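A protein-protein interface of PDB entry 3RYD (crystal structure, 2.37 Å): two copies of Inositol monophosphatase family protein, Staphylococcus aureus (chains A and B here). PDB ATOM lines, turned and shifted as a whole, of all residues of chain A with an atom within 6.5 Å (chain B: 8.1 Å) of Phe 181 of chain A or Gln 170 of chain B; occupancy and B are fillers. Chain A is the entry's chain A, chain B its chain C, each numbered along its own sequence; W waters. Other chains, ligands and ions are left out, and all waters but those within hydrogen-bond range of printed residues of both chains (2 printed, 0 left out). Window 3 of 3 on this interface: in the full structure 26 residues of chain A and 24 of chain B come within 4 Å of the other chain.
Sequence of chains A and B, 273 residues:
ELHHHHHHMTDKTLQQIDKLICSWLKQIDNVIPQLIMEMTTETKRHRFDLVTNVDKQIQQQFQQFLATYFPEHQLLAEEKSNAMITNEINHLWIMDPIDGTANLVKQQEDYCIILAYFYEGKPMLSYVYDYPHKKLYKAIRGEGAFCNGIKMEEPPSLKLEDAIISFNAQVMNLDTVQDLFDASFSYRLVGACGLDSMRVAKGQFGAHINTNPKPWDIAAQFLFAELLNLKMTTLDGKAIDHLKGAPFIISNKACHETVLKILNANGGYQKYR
Phe 181 of chain A touches two residues of chain B.
Of the printed residues of chain B, Ala 169 of chain A touches Phe 181.
Of the printed residues of chain A, Phe 181 of chain B touches Ala 169 (3.5 Å).
Of the printed residues of chain A, Tyr 187 of chain B touches Tyr 187.
Of the printed residues of chain B, Tyr 187 of chain A touches Gln 170, Tyr 187 and Leu 189.
Water W2 lies within hydrogen-bond range of OG of Ser 184 of chain A (2.5 Å), O of Phe 181 of chain A (2.8 Å), N of Ser 186 of chain A (3.2 Å) and OE1 of Gln 170 of chain B (3.4 Å).
Water W1 lies within hydrogen-bond range of NE2 of Gln 170 of chain B (2.6 Å), O of Phe 181 of chain A (3.1 Å) and O of Phe 185 of chain A (3.4 Å).
The side-chain amino group (NZ) of Lys 271 of chain B sits close to the side-chain amide nitrogen (NE2) of Gln 178 of chain A, 2.8 Å away.
The backbone carbonyl oxygen (O) of Phe 181 of chain A sits at hydrogen-bond distance from the side-chain amide nitrogen (NE2) of Gln 170 of chain B (3.4 Å).
Of the 14 printed residues of chain B, 6 touch a printed residue of chain A.
Printed residues of chain B that touch a printed residue of chain A: Ala 169, Gln 170, Phe 181, Tyr 187, Leu 189 and Lys 271.
Hydrophobic or aromatic side chains of chain B within 4 Å of the printed part of chain A: Phe 181, Tyr 187 and Leu 189.
Along chain B the printed residues that touch a printed residue of chain A span positions 169 to 271.
Printed residues of chain A that touch a printed residue of chain B: Ala 169, Gln 178, Phe 181, Ser 186 and Tyr 187.
Hydrophobic or aromatic side chains of chain A that line the printed part of chain B: Ala 169, Phe 181 and Tyr 187.
Among the printed residues, merely in contact across the chains: Ala 169 of chain A with Phe 181 of chain B (3.5 Å), Tyr 187 of chain A with Leu 189 of chain B (3.5 Å), Tyr 187 of chain A with Tyr 187 of chain B (3.5 Å), Phe 181 of chain A with Ala 169 of chain B (3.8 Å), Tyr 187 of chain A with Gln 170 of chain B (3.8 Å) and Ser 186 of chain A with Gln 170 of chain B (3.9 Å).
N of Ile 165 of chain A sits at hydrogen-bond distance from O of Ser 186 of chain A, at 3.1 Å.
The backbone carbonyl oxygen of Phe 167 of chain A is in hydrogen-bond range of the side-chain hydroxyl of Tyr 187 of chain A (2.6 Å).
The backbone carbonyl oxygen (O) of Ser 186 of chain A sits at hydrogen-bond distance from the side-chain hydroxyl (OG) of Ser 184 of chain A (3.5 Å).
The side-chain hydroxyl of Tyr 187 of chain B is in hydrogen-bond range of the backbone carbonyl oxygen of Phe 167 of chain B, at 2.8 Å.
N of Gln 170 of chain B is in hydrogen-bond range of OD1 of Asn 168 of chain B (3.0 Å).
Ala 169 of chain A touches Phe 181 of chain B, and with the chains exchanged Phe 181 of chain A touches Ala 169 of chain B.
Tyr 187 of chain B touches its own counterpart, Tyr 187 of chain A.
Positions printed for both chains: 167, 169, 177, 181 and 187.
Of the 8 pairs that touch across the chains among the printed residues, 3 have their exchanged pair printed and touching as well.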
ATOM      1  N   ILE A 165     -16.038  -1.447   2.019  1.00  0.00           N
ATOM      2  CA  ILE A 165     -17.146  -0.714   1.432  1.00  0.00           C
ATOM      3  C   ILE A 165     -17.757  -1.452   0.233  1.00  0.00           C
ATOM      4  O   ILE A 165     -17.165  -2.374  -0.321  1.00  0.00           O
ATOM      5  CB  ILE A 165     -16.761   0.714   1.086  1.00  0.00           C
ATOM      6  CG1 ILE A 165     -15.702   0.704  -0.024  1.00  0.00           C
ATOM      7  CG2 ILE A 165     -16.274   1.408   2.368  1.00  0.00           C
ATOM      8  CD1 ILE A 165     -15.374   2.044  -0.546  1.00  0.00           C
ATOM      9  N   PHE A 167     -20.259  -0.603  -3.385  1.00  0.00           N
ATOM     10  CA  PHE A 167     -20.804   0.339  -4.355  1.00  0.00           C
ATOM     11  C   PHE A 167     -20.629  -0.281  -5.709  1.00  0.00           C
ATOM     12  O   PHE A 167     -19.853  -1.263  -5.875  1.00  0.00           O
ATOM     13  CB  PHE A 167     -20.086   1.700  -4.310  1.00  0.00           C
ATOM     14  CG  PHE A 167     -18.577   1.644  -4.603  1.00  0.00           C
ATOM     15  CD1 PHE A 167     -18.087   1.782  -5.915  1.00  0.00           C
ATOM     16  CD2 PHE A 167     -17.652   1.502  -3.554  1.00  0.00           C
ATOM     17  CE1 PHE A 167     -16.675   1.763  -6.179  1.00  0.00           C
ATOM     18  CE2 PHE A 167     -16.256   1.455  -3.810  1.00  0.00           C
ATOM     19  CZ  PHE A 167     -15.763   1.585  -5.106  1.00  0.00           C
ATOM     20  N   ALA A 169     -19.059  -0.170  -8.982  1.00  0.00           N
ATOM     21  CA  ALA A 169     -17.820   0.310  -9.582  1.00  0.00           C
ATOM     22  C   ALA A 169     -17.948   0.704 -11.068  1.00  0.00           C
ATOM     23  O   ALA A 169     -16.959   1.069 -11.729  1.00  0.00           O
ATOM     24  CB  ALA A 169     -16.737  -0.754  -9.418  1.00  0.00           C
ATOM     25  N   THR A 176     -12.345   7.951  -9.196  1.00  0.00           N
ATOM     26  CA  THR A 176     -13.059   7.880  -7.926  1.00  0.00           C
ATOM     27  C   THR A 176     -13.073   6.439  -7.374  1.00  0.00           C
ATOM     28  O   THR A 176     -12.973   6.230  -6.178  1.00  0.00           O
ATOM     29  CB  THR A 176     -14.514   8.389  -8.081  1.00  0.00           C
ATOM     30  OG1 THR A 176     -14.491   9.728  -8.572  1.00  0.00           O
ATOM     31  CG2 THR A 176     -15.288   8.358  -6.755  1.00  0.00           C
ATOM     32  N   VAL A 177     -13.189   5.464  -8.265  1.00  0.00           N
ATOM     33  CA  VAL A 177     -13.221   4.048  -7.900  1.00  0.00           C
ATOM     34  C   VAL A 177     -11.876   3.601  -7.320  1.00  0.00           C
ATOM     35  O   VAL A 177     -11.827   2.845  -6.325  1.00  0.00           O
ATOM     36  CB  VAL A 177     -13.619   3.166  -9.107  1.00  0.00           C
ATOM     37  CG1 VAL A 177     -13.428   1.677  -8.780  1.00  0.00           C
ATOM     38  CG2 VAL A 177     -15.061   3.432  -9.478  1.00  0.00           C
ATOM     39  N   GLN A 178     -10.803   4.072  -7.942  1.00  0.00           N
ATOM     40  CA  GLN A 178      -9.444   3.905  -7.430  1.00  0.00           C
ATOM     41  C   GLN A 178      -9.229   4.578  -6.065  1.00  0.00           C
ATOM     42  O   GLN A 178      -8.737   3.931  -5.126  1.00  0.00           O
ATOM     43  CB  GLN A 178      -8.435   4.454  -8.434  1.00  0.00           C
ATOM     44  CG  GLN A 178      -6.963   4.168  -8.112  1.00  0.00           C
ATOM     45  CD  GLN A 178      -6.542   2.759  -8.456  1.00  0.00           C
ATOM     46  OE1 GLN A 178      -6.807   1.817  -7.707  1.00  0.00           O
ATOM     47  NE2 GLN A 178      -5.849   2.613  -9.578  1.00  0.00           N
ATOM     48  N   ASP A 179      -9.603   5.854  -5.934  1.00  0.00           N
ATOM     49  CA  ASP A 179      -9.343   6.536  -4.669  1.00  0.00           C
ATOM     50  C   ASP A 179     -10.019   5.772  -3.540  1.00  0.00           C
ATOM     51  O   ASP A 179      -9.425   5.548  -2.486  1.00  0.00           O
ATOM     52  CB  ASP A 179      -9.806   7.991  -4.656  1.00  0.00           C
ATOM     53  CG  ASP A 179      -9.130   8.842  -5.705  1.00  0.00           C
ATOM     54  OD1 ASP A 179      -7.945   8.592  -6.027  1.00  0.00           O
ATOM     55  OD2 ASP A 179      -9.813   9.768  -6.222  1.00  0.00           O
ATOM     56  N   LEU A 180     -11.248   5.336  -3.807  1.00  0.00           N
ATOM     57  CA  LEU A 180     -12.035   4.592  -2.860  1.00  0.00           C
ATOM     58  C   LEU A 180     -11.439   3.193  -2.606  1.00  0.00           C
ATOM     59  O   LEU A 180     -11.551   2.639  -1.502  1.00  0.00           O
ATOM     60  CB  LEU A 180     -13.458   4.487  -3.388  1.00  0.00           C
ATOM     61  CG  LEU A 180     -14.368   5.721  -3.432  1.00  0.00           C
ATOM     62  CD1 LEU A 180     -15.697   5.301  -4.130  1.00  0.00           C
ATOM     63  CD2 LEU A 180     -14.655   6.227  -2.042  1.00  0.00           C
ATOM     64  N   PHE A 181     -10.795   2.645  -3.623  1.00  0.00           N
ATOM     65  CA  PHE A 181     -10.086   1.413  -3.462  1.00  0.00           C
ATOM     66  C   PHE A 181      -8.939   1.610  -2.491  1.00  0.00           C
ATOM     67  O   PHE A 181      -8.764   0.801  -1.568  1.00  0.00           O
ATOM     68  CB  PHE A 181      -9.564   0.910  -4.803  1.00  0.00           C
ATOM     69  CG  PHE A 181     -10.589   0.158  -5.618  1.00  0.00           C
ATOM     70  CD1 PHE A 181     -11.846  -0.137  -5.094  1.00  0.00           C
ATOM     71  CD2 PHE A 181     -10.262  -0.317  -6.873  1.00  0.00           C
ATOM     72  CE1 PHE A 181     -12.777  -0.858  -5.808  1.00  0.00           C
ATOM     73  CE2 PHE A 181     -11.186  -1.060  -7.617  1.00  0.00           C
ATOM     74  CZ  PHE A 181     -12.456  -1.324  -7.084  1.00  0.00           C
ATOM     75  N   ASP A 182      -8.187   2.701  -2.692  1.00  0.00           N
ATOM     76  CA  ASP A 182      -7.026   3.066  -1.873  1.00  0.00           C
ATOM     77  C   ASP A 182      -7.346   3.419  -0.439  1.00  0.00           C
ATOM     78  O   ASP A 182      -6.608   3.019   0.485  1.00  0.00           O
ATOM     79  CB  ASP A 182      -6.278   4.245  -2.487  1.00  0.00           C
ATOM     80  CG  ASP A 182      -5.669   3.911  -3.832  1.00  0.00           C
ATOM     81  OD1 ASP A 182      -5.753   2.736  -4.247  1.00  0.00           O
ATOM     82  OD2 ASP A 182      -5.109   4.825  -4.482  1.00  0.00           O
ATOM     83  N   ALA A 183      -8.424   4.177  -0.242  1.00  0.00           N
ATOM     84  CA  ALA A 183      -8.737   4.718   1.086  1.00  0.00           C
ATOM     85  C   ALA A 183      -9.447   3.709   2.003  1.00  0.00           C
ATOM     86  O   ALA A 183      -9.378   3.833   3.221  1.00  0.00           O
ATOM     87  CB  ALA A 183      -9.529   6.032   0.975  1.00  0.00           C
ATOM     88  N   SER A 184     -10.105   2.703   1.420  1.00  0.00           N
ATOM     89  CA  SER A 184     -10.841   1.703   2.199  1.00  0.00           C
ATOM     90  C   SER A 184     -10.026   0.449   2.432  1.00  0.00           C
ATOM     91  O   SER A 184      -8.954   0.274   1.845  1.00  0.00           O
ATOM     92  CB  SER A 184     -12.146   1.355   1.505  1.00  0.00           C
ATOM     93  OG  SER A 184     -11.864   0.731   0.273  1.00  0.00           O
ATOM     94  N   PHE A 185     -10.516  -0.409   3.322  1.00  0.00           N
ATOM     95  CA  PHE A 185      -9.814  -1.639   3.653  1.00  0.00           C
ATOM     96  C   PHE A 185      -9.915  -2.632   2.524  1.00  0.00           C
ATOM     97  O   PHE A 185      -8.927  -3.280   2.129  1.00  0.00           O
ATOM     98  CB  PHE A 185     -10.393  -2.305   4.882  1.00  0.00           C
ATOM     99  CG  PHE A 185      -9.687  -3.528   5.224  1.00  0.00           C
ATOM    100  CD1 PHE A 185      -8.428  -3.455   5.819  1.00  0.00           C
ATOM    101  CD2 PHE A 185     -10.191  -4.757   4.854  1.00  0.00           C
ATOM    102  CE1 PHE A 185      -7.712  -4.613   6.118  1.00  0.00           C
ATOM    103  CE2 PHE A 185      -9.489  -5.919   5.143  1.00  0.00           C
ATOM    104  CZ  PHE A 185      -8.245  -5.849   5.776  1.00  0.00           C
ATOM    105  N   SER A 186     -11.144  -2.775   2.033  1.00  0.00           N
ATOM    106  CA  SER A 186     -11.395  -3.639   0.930  1.00  0.00           C
ATOM    107  C   SER A 186     -12.722  -3.283   0.329  1.00  0.00           C
ATOM    108  O   SER A 186     -13.386  -2.350   0.781  1.00  0.00           O
ATOM    109  CB  SER A 186     -11.362  -5.113   1.346  1.00  0.00           C
ATOM    110  OG  SER A 186     -11.281  -5.883   0.171  1.00  0.00           O
ATOM    111  N   TYR A 187     -13.080  -4.040  -0.706  1.00  0.00           N
ATOM    112  CA  TYR A 187     -14.277  -3.804  -1.463  1.00  0.00           C
ATOM    113  C   TYR A 187     -15.017  -5.111  -1.745  1.00  0.00           C
ATOM    114  O   TYR A 187     -14.421  -6.109  -2.168  1.00  0.00           O
ATOM    115  CB  TYR A 187     -13.904  -3.126  -2.778  1.00  0.00           C
ATOM    116  CG  TYR A 187     -14.986  -3.154  -3.795  1.00  0.00           C
ATOM    117  CD1 TYR A 187     -15.932  -2.146  -3.808  1.00  0.00           C
ATOM    118  CD2 TYR A 187     -15.088  -4.206  -4.740  1.00  0.00           C
ATOM    119  CE1 TYR A 187     -16.931  -2.125  -4.717  1.00  0.00           C
ATOM    120  CE2 TYR A 187     -16.110  -4.190  -5.682  1.00  0.00           C
ATOM    121  CZ  TYR A 187     -17.043  -3.135  -5.660  1.00  0.00           C
ATOM    122  OH  TYR A 187     -18.106  -3.043  -6.563  1.00  0.00           O
ATOM    123  N   PHE B 167     -14.187 -11.037  -9.746  1.00  0.00           N
ATOM    124  CA  PHE B 167     -12.747 -10.930  -9.665  1.00  0.00           C
ATOM    125  C   PHE B 167     -12.362  -9.807  -8.711  1.00  0.00           C
ATOM    126  O   PHE B 167     -13.194  -8.944  -8.364  1.00  0.00           O
ATOM    127  CB  PHE B 167     -12.145 -10.650 -11.036  1.00  0.00           C
ATOM    128  CG  PHE B 167     -12.751  -9.445 -11.772  1.00  0.00           C
ATOM    129  CD1 PHE B 167     -12.148  -8.199 -11.691  1.00  0.00           C
ATOM    130  CD2 PHE B 167     -13.889  -9.590 -12.574  1.00  0.00           C
ATOM    131  CE1 PHE B 167     -12.670  -7.080 -12.354  1.00  0.00           C
ATOM    132  CE2 PHE B 167     -14.428  -8.487 -13.267  1.00  0.00           C
ATOM    133  CZ  PHE B 167     -13.809  -7.210 -13.164  1.00  0.00           C
ATOM    134  N   ASN B 168     -11.093  -9.805  -8.281  1.00  0.00           N
ATOM    135  CA  ASN B 168     -10.546  -8.633  -7.584  1.00  0.00           C
ATOM    136  C   ASN B 168     -10.196  -7.545  -8.584  1.00  0.00           C
ATOM    137  O   ASN B 168      -9.191  -7.620  -9.282  1.00  0.00           O
ATOM    138  CB  ASN B 168      -9.351  -8.990  -6.697  1.00  0.00           C
ATOM    139  CG  ASN B 168      -8.889  -7.813  -5.807  1.00  0.00           C
ATOM    140  OD1 ASN B 168      -9.443  -6.705  -5.846  1.00  0.00           O
ATOM    141  ND2 ASN B 168      -7.855  -8.061  -5.014  1.00  0.00           N
ATOM    142  N   ALA B 169     -11.028  -6.518  -8.631  1.00  0.00           N
ATOM    143  CA  ALA B 169     -10.804  -5.404  -9.548  1.00  0.00           C
ATOM    144  C   ALA B 169      -9.688  -4.414  -9.135  1.00  0.00           C
ATOM    145  O   ALA B 169      -9.372  -3.521  -9.923  1.00  0.00           O
ATOM    146  CB  ALA B 169     -12.129  -4.644  -9.804  1.00  0.00           C
ATOM    147  N   GLN B 170      -9.111  -4.554  -7.924  1.00  0.00           N
ATOM    148  CA  GLN B 170      -8.105  -3.568  -7.407  1.00  0.00           C
ATOM    149  C   GLN B 170      -6.699  -3.943  -7.844  1.00  0.00           C
ATOM    150  O   GLN B 170      -5.727  -3.279  -7.507  1.00  0.00           O
ATOM    151  CB  GLN B 170      -8.090  -3.457  -5.870  1.00  0.00           C
ATOM    152  CG  GLN B 170      -9.437  -3.506  -5.143  1.00  0.00           C
ATOM    153  CD  GLN B 170      -9.308  -3.122  -3.665  1.00  0.00           C
ATOM    154  OE1 GLN B 170      -9.865  -3.772  -2.789  1.00  0.00           O
ATOM    155  NE2 GLN B 170      -8.593  -2.046  -3.400  1.00  0.00           N
ATOM    156  N   VAL B 171      -6.601  -5.021  -8.604  1.00  0.00           N
ATOM    157  CA  VAL B 171      -5.336  -5.687  -8.793  1.00  0.00           C
ATOM    158  C   VAL B 171      -5.076  -5.880 -10.279  1.00  0.00           C
ATOM    159  O   VAL B 171      -4.021  -6.370 -10.689  1.00  0.00           O
ATOM    160  CB  VAL B 171      -5.359  -6.964  -7.929  1.00  0.00           C
ATOM    161  CG1 VAL B 171      -5.243  -8.248  -8.729  1.00  0.00           C
ATOM    162  CG2 VAL B 171      -4.369  -6.838  -6.792  1.00  0.00           C
ATOM    163  N   MET B 172      -6.040  -5.436 -11.078  1.00  0.00           N
ATOM    164  CA  MET B 172      -5.947  -5.451 -12.537  1.00  0.00           C
ATOM    165  C   MET B 172      -5.878  -4.033 -13.109  1.00  0.00           C
ATOM    166  O   MET B 172      -6.357  -3.062 -12.478  1.00  0.00           O
ATOM    167  CB  MET B 172      -7.136  -6.178 -13.159  1.00  0.00           C
ATOM    168  CG  MET B 172      -7.120  -7.656 -12.981  1.00  0.00           C
ATOM    169  SD  MET B 172      -8.689  -8.231 -13.580  1.00  0.00           S
ATOM    170  CE  MET B 172      -8.730  -9.923 -13.009  1.00  0.00           C
ATOM    171  N   ASN B 173      -5.265  -3.897 -14.291  1.00  0.00           N
ATOM    172  CA  ASN B 173      -5.224  -2.593 -14.912  1.00  0.00           C
ATOM    173  C   ASN B 173      -6.625  -2.144 -15.351  1.00  0.00           C
ATOM    174  O   ASN B 173      -7.424  -2.936 -15.863  1.00  0.00           O
ATOM    175  CB  ASN B 173      -4.181  -2.505 -16.030  1.00  0.00           C
ATOM    176  CG  ASN B 173      -4.490  -3.398 -17.199  1.00  0.00           C
ATOM    177  OD1 ASN B 173      -5.422  -3.138 -17.947  1.00  0.00           O
ATOM    178  ND2 ASN B 173      -3.670  -4.437 -17.398  1.00  0.00           N
ATOM    179  N   LEU B 174      -6.891  -0.859 -15.118  1.00  0.00           N
ATOM    180  CA  LEU B 174      -8.179  -0.209 -15.366  1.00  0.00           C
ATOM    181  C   LEU B 174      -8.853  -0.547 -16.695  1.00  0.00           C
ATOM    182  O   LEU B 174     -10.073  -0.697 -16.744  1.00  0.00           O
ATOM    183  CB  LEU B 174      -8.021   1.305 -15.201  1.00  0.00           C
ATOM    184  CG  LEU B 174      -8.109   1.852 -13.762  1.00  0.00           C
ATOM    185  CD1 LEU B 174      -8.227   0.766 -12.654  1.00  0.00           C
ATOM    186  CD2 LEU B 174      -6.948   2.866 -13.467  1.00  0.00           C
ATOM    187  N   VAL B 177     -10.176  -3.965 -16.368  1.00  0.00           N
ATOM    188  CA  VAL B 177     -11.396  -3.757 -15.571  1.00  0.00           C
ATOM    189  C   VAL B 177     -12.581  -3.259 -16.380  1.00  0.00           C
ATOM    190  O   VAL B 177     -13.626  -3.895 -16.381  1.00  0.00           O
ATOM    191  CB  VAL B 177     -11.146  -2.909 -14.325  1.00  0.00           C
ATOM    192  CG1 VAL B 177     -12.443  -2.595 -13.634  1.00  0.00           C
ATOM    193  CG2 VAL B 177     -10.237  -3.697 -13.365  1.00  0.00           C
ATOM    194  N   PHE B 181     -16.254  -5.224 -17.333  1.00  0.00           N
ATOM    195  CA  PHE B 181     -17.539  -4.655 -16.947  1.00  0.00           C
ATOM    196  C   PHE B 181     -18.433  -4.601 -18.174  1.00  0.00           C
ATOM    197  O   PHE B 181     -19.559  -5.096 -18.110  1.00  0.00           O
ATOM    198  CB  PHE B 181     -17.371  -3.261 -16.348  1.00  0.00           C
ATOM    199  CG  PHE B 181     -16.859  -3.253 -14.938  1.00  0.00           C
ATOM    200  CD1 PHE B 181     -16.802  -4.423 -14.177  1.00  0.00           C
ATOM    201  CD2 PHE B 181     -16.490  -2.059 -14.350  1.00  0.00           C
ATOM    202  CE1 PHE B 181     -16.355  -4.393 -12.883  1.00  0.00           C
ATOM    203  CE2 PHE B 181     -16.022  -2.025 -13.047  1.00  0.00           C
ATOM    204  CZ  PHE B 181     -15.966  -3.187 -12.311  1.00  0.00           C
ATOM    205  N   TYR B 187     -21.189  -7.463 -12.404  1.00  0.00           N
ATOM    206  CA  TYR B 187     -20.043  -7.781 -11.594  1.00  0.00           C
ATOM    207  C   TYR B 187     -20.510  -7.945 -10.154  1.00  0.00           C
ATOM    208  O   TYR B 187     -21.343  -7.174  -9.680  1.00  0.00           O
ATOM    209  CB  TYR B 187     -19.024  -6.639 -11.703  1.00  0.00           C
ATOM    210  CG  TYR B 187     -17.890  -6.692 -10.697  1.00  0.00           C
ATOM    211  CD1 TYR B 187     -16.819  -7.579 -10.842  1.00  0.00           C
ATOM    212  CD2 TYR B 187     -17.878  -5.837  -9.627  1.00  0.00           C
ATOM    213  CE1 TYR B 187     -15.768  -7.612  -9.905  1.00  0.00           C
ATOM    214  CE2 TYR B 187     -16.860  -5.862  -8.696  1.00  0.00           C
ATOM    215  CZ  TYR B 187     -15.806  -6.747  -8.831  1.00  0.00           C
ATOM    216  OH  TYR B 187     -14.814  -6.694  -7.879  1.00  0.00           O
ATOM    217  N   LEU B 189     -18.876  -9.597  -6.083  1.00  0.00           N
ATOM    218  CA  LEU B 189     -17.735 -10.199  -5.368  1.00  0.00           C
ATOM    219  C   LEU B 189     -18.115 -10.625  -3.963  1.00  0.00           C
ATOM    220  O   LEU B 189     -18.568  -9.807  -3.182  1.00  0.00           O
ATOM    221  CB  LEU B 189     -16.532  -9.234  -5.304  1.00  0.00           C
ATOM    222  CG  LEU B 189     -15.264  -9.824  -4.626  1.00  0.00           C
ATOM    223  CD1 LEU B 189     -14.716 -11.032  -5.426  1.00  0.00           C
ATOM    224  CD2 LEU B 189     -14.179  -8.767  -4.430  1.00  0.00           C
ATOM    225  N   LYS B 271      -1.693  -4.778 -13.338  1.00  0.00           N
ATOM    226  CA  LYS B 271      -1.789  -3.381 -12.962  1.00  0.00           C
ATOM    227  C   LYS B 271      -0.406  -2.810 -12.681  1.00  0.00           C
ATOM    228  O   LYS B 271       0.403  -3.408 -11.971  1.00  0.00           O
ATOM    229  CB  LYS B 271      -2.678  -3.209 -11.713  1.00  0.00           C
ATOM    230  CG  LYS B 271      -3.161  -1.771 -11.486  1.00  0.00           C
ATOM    231  CD  LYS B 271      -3.069  -1.362 -10.024  1.00  0.00           C
ATOM    232  CE  LYS B 271      -4.421  -1.218  -9.369  1.00  0.00           C
ATOM    233  NZ  LYS B 271      -5.216  -0.105  -9.960  1.00  0.00           N
ATOM    234  N   ARG B 273       1.350   1.105 -11.756  1.00  0.00           N
ATOM    235  CA  ARG B 273       1.196   2.517 -11.401  1.00  0.00           C
ATOM    236  C   ARG B 273      -0.106   2.782 -10.621  1.00  0.00           C
ATOM    237  O   ARG B 273      -0.676   1.889  -9.975  1.00  0.00           O
ATOM    238  CB  ARG B 273       1.367   3.422 -12.654  1.00  0.00           C
ATOM    239  CG  ARG B 273       0.131   4.226 -13.167  1.00  0.00           C
ATOM    240  CD  ARG B 273       0.124   5.684 -12.645  1.00  0.00           C
ATOM    241  NE  ARG B 273       1.490   6.195 -12.492  1.00  0.00           N
ATOM    242  CZ  ARG B 273       2.237   6.100 -11.385  1.00  0.00           C
ATOM    243  NH1 ARG B 273       1.775   5.531 -10.278  1.00  0.00           N
ATOM    244  NH2 ARG B 273       3.468   6.580 -11.389  1.00  0.00           N
HETATM  245  O   HOH W   1      -7.858  -2.145  -0.935  1.00  0.00           O
HETATM  246  O   HOH W   2     -10.504  -1.158  -0.680  1.00  0.00           O
